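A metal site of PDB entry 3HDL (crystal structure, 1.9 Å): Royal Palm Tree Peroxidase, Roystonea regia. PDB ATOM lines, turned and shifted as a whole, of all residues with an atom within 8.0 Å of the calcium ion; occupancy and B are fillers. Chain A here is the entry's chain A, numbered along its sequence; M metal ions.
The side-chain carboxylate (OD1) of Asp 223 is in hydrogen-bond range of the backbone NH (N) of Ile 225.
N of Met 233 sits close to OD1 of Asp 231, 3.2 Å away.
The calcium ion is bound by OD2 of Asp 223 (2.4 Å), O of Thr 226 (2.4 Å), O of Val 229 (2.4 Å), O of Ser 170 (2.5 Å), OG of Ser 170 (2.5 Å), OG1 of Thr 226 (2.5 Å) and OD1 of Asp 231 (2.6 Å).
The calcium ion has seven donor atoms within binding distance.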
ATOM      1  N   ALA A 112      11.700 -17.403 -12.213  1.00  0.00           N
ATOM      2  CA  ALA A 112      13.169 -17.450 -12.239  1.00  0.00           C
ATOM      3  C   ALA A 112      13.791 -18.333 -11.163  1.00  0.00           C
ATOM      4  O   ALA A 112      14.921 -18.797 -11.319  1.00  0.00           O
ATOM      5  CB  ALA A 112      13.739 -16.028 -12.147  1.00  0.00           C
ATOM      6  N   GLY A 167      20.453 -10.460  -3.084  1.00  0.00           N
ATOM      7  CA  GLY A 167      20.414 -11.765  -3.734  1.00  0.00           C
ATOM      8  C   GLY A 167      19.600 -11.774  -5.007  1.00  0.00           C
ATOM      9  O   GLY A 167      19.627 -12.748  -5.764  1.00  0.00           O
ATOM     10  N   ALA A 168      18.864 -10.695  -5.268  1.00  0.00           N
ATOM     11  CA  ALA A 168      18.193 -10.540  -6.563  1.00  0.00           C
ATOM     12  C   ALA A 168      19.224 -10.506  -7.694  1.00  0.00           C
ATOM     13  O   ALA A 168      18.888 -10.786  -8.857  1.00  0.00           O
ATOM     14  CB  ALA A 168      17.350  -9.266  -6.575  1.00  0.00           C
ATOM     15  N   HIS A 169      20.471 -10.167  -7.365  1.00  0.00           N
ATOM     16  CA  HIS A 169      21.555 -10.153  -8.352  1.00  0.00           C
ATOM     17  C   HIS A 169      21.983 -11.569  -8.711  1.00  0.00           C
ATOM     18  O   HIS A 169      22.972 -11.768  -9.430  1.00  0.00           O
ATOM     19  CB  HIS A 169      22.766  -9.351  -7.855  1.00  0.00           C
ATOM     20  CG  HIS A 169      22.492  -7.882  -7.735  1.00  0.00           C
ATOM     21  ND1 HIS A 169      23.408  -7.002  -7.190  1.00  0.00           N
ATOM     22  CD2 HIS A 169      21.412  -7.148  -8.071  1.00  0.00           C
ATOM     23  CE1 HIS A 169      22.898  -5.789  -7.207  1.00  0.00           C
ATOM     24  NE2 HIS A 169      21.686  -5.842  -7.727  1.00  0.00           N
ATOM     25  N   SER A 170      21.258 -12.549  -8.197  1.00  0.00           N
ATOM     26  CA  SER A 170      21.481 -13.928  -8.582  1.00  0.00           C
ATOM     27  C   SER A 170      20.994 -14.173 -10.005  1.00  0.00           C
ATOM     28  O   SER A 170      21.226 -15.227 -10.578  1.00  0.00           O
ATOM     29  CB  SER A 170      20.783 -14.875  -7.612  1.00  0.00           C
ATOM     30  OG  SER A 170      21.346 -16.163  -7.684  1.00  0.00           O
ATOM     31  N   ILE A 171      20.283 -13.196 -10.565  1.00  0.00           N
ATOM     32  CA  ILE A 171      19.844 -13.262 -11.958  1.00  0.00           C
ATOM     33  C   ILE A 171      20.082 -11.905 -12.610  1.00  0.00           C
ATOM     34  O   ILE A 171      20.433 -10.948 -11.938  1.00  0.00           O
ATOM     35  CB  ILE A 171      18.330 -13.577 -12.087  1.00  0.00           C
ATOM     36  CG1 ILE A 171      17.500 -12.614 -11.231  1.00  0.00           C
ATOM     37  CG2 ILE A 171      18.041 -15.041 -11.723  1.00  0.00           C
ATOM     38  CD1 ILE A 171      15.988 -12.782 -11.383  1.00  0.00           C
ATOM     39  N   GLY A 172      19.909 -11.827 -13.922  1.00  0.00           N
ATOM     40  CA  GLY A 172      19.975 -10.552 -14.608  1.00  0.00           C
ATOM     41  C   GLY A 172      21.388 -10.081 -14.916  1.00  0.00           C
ATOM     42  O   GLY A 172      22.359 -10.809 -14.714  1.00  0.00           O
ATOM     43  N   LEU A 222      25.191 -10.819 -13.717  1.00  0.00           N
ATOM     44  CA  LEU A 222      25.615 -10.519 -12.360  1.00  0.00           C
ATOM     45  C   LEU A 222      26.143 -11.748 -11.617  1.00  0.00           C
ATOM     46  O   LEU A 222      27.069 -11.651 -10.815  1.00  0.00           O
ATOM     47  CB  LEU A 222      24.459  -9.887 -11.575  1.00  0.00           C
ATOM     48  CG  LEU A 222      24.186  -8.411 -11.913  1.00  0.00           C
ATOM     49  CD1 LEU A 222      22.746  -8.013 -11.607  1.00  0.00           C
ATOM     50  CD2 LEU A 222      25.163  -7.508 -11.160  1.00  0.00           C
ATOM     51  N   ASP A 223      25.532 -12.891 -11.889  1.00  0.00           N
ATOM     52  CA  ASP A 223      25.929 -14.134 -11.233  1.00  0.00           C
ATOM     53  C   ASP A 223      26.563 -15.071 -12.241  1.00  0.00           C
ATOM     54  O   ASP A 223      25.873 -15.615 -13.107  1.00  0.00           O
ATOM     55  CB  ASP A 223      24.723 -14.815 -10.592  1.00  0.00           C
ATOM     56  CG  ASP A 223      25.073 -16.156  -9.950  1.00  0.00           C
ATOM     57  OD1 ASP A 223      26.262 -16.481  -9.792  1.00  0.00           O
ATOM     58  OD2 ASP A 223      24.141 -16.888  -9.592  1.00  0.00           O
ATOM     59  N   ILE A 224      27.877 -15.259 -12.150  1.00  0.00           N
ATOM     60  CA  ILE A 224      28.596 -16.063 -13.128  1.00  0.00           C
ATOM     61  C   ILE A 224      28.308 -17.552 -12.942  1.00  0.00           C
ATOM     62  O   ILE A 224      28.577 -18.353 -13.835  1.00  0.00           O
ATOM     63  CB  ILE A 224      30.124 -15.808 -13.058  1.00  0.00           C
ATOM     64  CG1 ILE A 224      30.815 -16.389 -14.301  1.00  0.00           C
ATOM     65  CG2 ILE A 224      30.702 -16.363 -11.765  1.00  0.00           C
ATOM     66  CD1 ILE A 224      32.309 -16.120 -14.360  1.00  0.00           C
ATOM     67  N   ILE A 225      27.754 -17.921 -11.786  1.00  0.00           N
ATOM     68  CA  ILE A 225      27.521 -19.334 -11.483  1.00  0.00           C
ATOM     69  C   ILE A 225      26.214 -19.843 -12.097  1.00  0.00           C
ATOM     70  O   ILE A 225      26.240 -20.726 -12.967  1.00  0.00           O
ATOM     71  CB  ILE A 225      27.567 -19.601  -9.967  1.00  0.00           C
ATOM     72  CG1 ILE A 225      28.959 -19.253  -9.420  1.00  0.00           C
ATOM     73  CG2 ILE A 225      27.237 -21.058  -9.678  1.00  0.00           C
ATOM     74  CD1 ILE A 225      29.048 -19.181  -7.910  1.00  0.00           C
ATOM     75  N   THR A 226      25.083 -19.293 -11.678  1.00  0.00           N
ATOM     76  CA  THR A 226      23.804 -19.629 -12.316  1.00  0.00           C
ATOM     77  C   THR A 226      23.083 -18.357 -12.773  1.00  0.00           C
ATOM     78  O   THR A 226      22.152 -17.895 -12.134  1.00  0.00           O
ATOM     79  CB  THR A 226      22.877 -20.469 -11.396  1.00  0.00           C
ATOM     80  OG1 THR A 226      22.732 -19.821 -10.128  1.00  0.00           O
ATOM     81  CG2 THR A 226      23.457 -21.861 -11.175  1.00  0.00           C
ATOM     82  N   PRO A 227      23.501 -17.785 -13.902  1.00  0.00           N
ATOM     83  CA  PRO A 227      23.019 -16.458 -14.320  1.00  0.00           C
ATOM     84  C   PRO A 227      21.504 -16.352 -14.518  1.00  0.00           C
ATOM     85  O   PRO A 227      20.990 -15.230 -14.476  1.00  0.00           O
ATOM     86  CB  PRO A 227      23.742 -16.238 -15.666  1.00  0.00           C
ATOM     87  CG  PRO A 227      24.084 -17.631 -16.125  1.00  0.00           C
ATOM     88  CD  PRO A 227      24.487 -18.310 -14.860  1.00  0.00           C
ATOM     89  N   SER A 228      20.792 -17.467 -14.710  1.00  0.00           N
ATOM     90  CA  SER A 228      19.358 -17.363 -14.970  1.00  0.00           C
ATOM     91  C   SER A 228      18.493 -18.045 -13.903  1.00  0.00           C
ATOM     92  O   SER A 228      17.274 -18.186 -14.077  1.00  0.00           O
ATOM     93  CB  SER A 228      19.007 -17.881 -16.358  1.00  0.00           C
ATOM     94  OG  SER A 228      19.171 -19.285 -16.445  1.00  0.00           O
ATOM     95  N   VAL A 229      19.108 -18.451 -12.799  1.00  0.00           N
ATOM     96  CA  VAL A 229      18.342 -19.045 -11.707  1.00  0.00           C
ATOM     97  C   VAL A 229      18.388 -18.135 -10.488  1.00  0.00           C
ATOM     98  O   VAL A 229      19.460 -17.782 -10.020  1.00  0.00           O
ATOM     99  CB  VAL A 229      18.895 -20.439 -11.306  1.00  0.00           C
ATOM    100  CG1 VAL A 229      18.036 -21.037 -10.193  1.00  0.00           C
ATOM    101  CG2 VAL A 229      18.939 -21.358 -12.526  1.00  0.00           C
ATOM    102  N   LEU A 230      17.220 -17.762  -9.976  1.00  0.00           N
ATOM    103  CA  LEU A 230      17.151 -16.957  -8.765  1.00  0.00           C
ATOM    104  C   LEU A 230      17.370 -17.856  -7.556  1.00  0.00           C
ATOM    105  O   LEU A 230      16.433 -18.295  -6.902  1.00  0.00           O
ATOM    106  CB  LEU A 230      15.812 -16.228  -8.692  1.00  0.00           C
ATOM    107  CG  LEU A 230      15.552 -15.280  -7.515  1.00  0.00           C
ATOM    108  CD1 LEU A 230      16.620 -14.202  -7.400  1.00  0.00           C
ATOM    109  CD2 LEU A 230      14.173 -14.638  -7.632  1.00  0.00           C
ATOM    110  N   ASP A 231      18.653 -18.138  -7.284  1.00  0.00           N
ATOM    111  CA  ASP A 231      19.039 -19.003  -6.181  1.00  0.00           C
ATOM    112  C   ASP A 231      20.061 -18.268  -5.317  1.00  0.00           C
ATOM    113  O   ASP A 231      20.258 -17.068  -5.475  1.00  0.00           O
ATOM    114  CB  ASP A 231      19.614 -20.325  -6.698  1.00  0.00           C
ATOM    115  CG  ASP A 231      20.774 -20.123  -7.671  1.00  0.00           C
ATOM    116  OD1 ASP A 231      21.310 -19.003  -7.714  1.00  0.00           O
ATOM    117  OD2 ASP A 231      21.140 -21.073  -8.386  1.00  0.00           O
ATOM    118  N   ASN A 232      20.719 -19.002  -4.429  1.00  0.00           N
ATOM    119  CA  ASN A 232      21.676 -18.397  -3.517  1.00  0.00           C
ATOM    120  C   ASN A 232      23.124 -18.402  -4.032  1.00  0.00           C
ATOM    121  O   ASN A 232      24.036 -18.075  -3.283  1.00  0.00           O
ATOM    122  CB  ASN A 232      21.601 -19.097  -2.149  1.00  0.00           C
ATOM    123  CG  ASN A 232      21.912 -20.579  -2.239  1.00  0.00           C
ATOM    124  OD1 ASN A 232      21.682 -21.210  -3.271  1.00  0.00           O
ATOM    125  ND2 ASN A 232      22.443 -21.137  -1.156  1.00  0.00           N
ATOM    126  N   MET A 233      23.329 -18.748  -5.304  1.00  0.00           N
ATOM    127  CA  MET A 233      24.681 -18.813  -5.849  1.00  0.00           C
ATOM    128  C   MET A 233      25.334 -17.439  -5.948  1.00  0.00           C
ATOM    129  O   MET A 233      26.559 -17.329  -6.044  1.00  0.00           O
ATOM    130  CB  MET A 233      24.706 -19.534  -7.206  1.00  0.00           C
ATOM    131  CG  MET A 233      24.485 -21.043  -7.122  1.00  0.00           C
ATOM    132  SD  MET A 233      25.785 -21.911  -6.205  1.00  0.00           S
ATOM    133  CE  MET A 233      25.165 -21.806  -4.521  1.00  0.00           C
ATOM    134  N   TYR A 234      24.519 -16.392  -5.923  1.00  0.00           N
ATOM    135  CA  TYR A 234      25.048 -15.031  -5.885  1.00  0.00           C
ATOM    136  C   TYR A 234      25.983 -14.894  -4.684  1.00  0.00           C
ATOM    137  O   TYR A 234      27.068 -14.319  -4.780  1.00  0.00           O
ATOM    138  CB  TYR A 234      23.907 -14.027  -5.769  1.00  0.00           C
ATOM    139  CG  TYR A 234      24.314 -12.648  -5.271  1.00  0.00           C
ATOM    140  CD1 TYR A 234      24.863 -11.707  -6.131  1.00  0.00           C
ATOM    141  CD2 TYR A 234      24.135 -12.296  -3.933  1.00  0.00           C
ATOM    142  CE1 TYR A 234      25.228 -10.451  -5.671  1.00  0.00           C
ATOM    143  CE2 TYR A 234      24.491 -11.038  -3.469  1.00  0.00           C
ATOM    144  CZ  TYR A 234      25.039 -10.128  -4.342  1.00  0.00           C
ATOM    145  OH  TYR A 234      25.388  -8.871  -3.890  1.00  0.00           O
ATOM    146  N   TYR A 235      25.562 -15.442  -3.547  1.00  0.00           N
ATOM    147  CA  TYR A 235      26.332 -15.357  -2.312  1.00  0.00           C
ATOM    148  C   TYR A 235      27.610 -16.170  -2.408  1.00  0.00           C
ATOM    149  O   TYR A 235      28.670 -15.722  -1.990  1.00  0.00           O
ATOM    150  CB  TYR A 235      25.478 -15.786  -1.118  1.00  0.00           C
ATOM    151  CG  TYR A 235      24.278 -14.894  -0.968  1.00  0.00           C
ATOM    152  CD1 TYR A 235      23.019 -15.317  -1.397  1.00  0.00           C
ATOM    153  CD2 TYR A 235      24.392 -13.625  -0.423  1.00  0.00           C
ATOM    154  CE1 TYR A 235      21.917 -14.496  -1.279  1.00  0.00           C
ATOM    155  CE2 TYR A 235      23.297 -12.803  -0.293  1.00  0.00           C
ATOM    156  CZ  TYR A 235      22.061 -13.242  -0.717  1.00  0.00           C
ATOM    157  OH  TYR A 235      20.965 -12.420  -0.588  1.00  0.00           O
ATOM    158  N   TRP A 271      17.513 -18.770   2.695  1.00  0.00           N
ATOM    159  CA  TRP A 271      17.606 -17.499   1.994  1.00  0.00           C
ATOM    160  C   TRP A 271      16.340 -17.191   1.204  1.00  0.00           C
ATOM    161  O   TRP A 271      15.834 -16.070   1.242  1.00  0.00           O
ATOM    162  CB  TRP A 271      18.812 -17.448   1.049  1.00  0.00           C
ATOM    163  CG  TRP A 271      18.684 -16.277   0.107  1.00  0.00           C
ATOM    164  CD1 TRP A 271      18.974 -14.969   0.376  1.00  0.00           C
ATOM    165  CD2 TRP A 271      18.205 -16.312  -1.242  1.00  0.00           C
ATOM    166  NE1 TRP A 271      18.701 -14.193  -0.727  1.00  0.00           N
ATOM    167  CE2 TRP A 271      18.225 -14.998  -1.733  1.00  0.00           C
ATOM    168  CE3 TRP A 271      17.748 -17.333  -2.085  1.00  0.00           C
ATOM    169  CZ2 TRP A 271      17.827 -14.661  -3.029  1.00  0.00           C
ATOM    170  CZ3 TRP A 271      17.352 -17.016  -3.372  1.00  0.00           C
ATOM    171  CH2 TRP A 271      17.394 -15.685  -3.829  1.00  0.00           C
HETATM  172 CA    CA M   1      21.863 -17.454  -9.771  1.00  0.00          CA
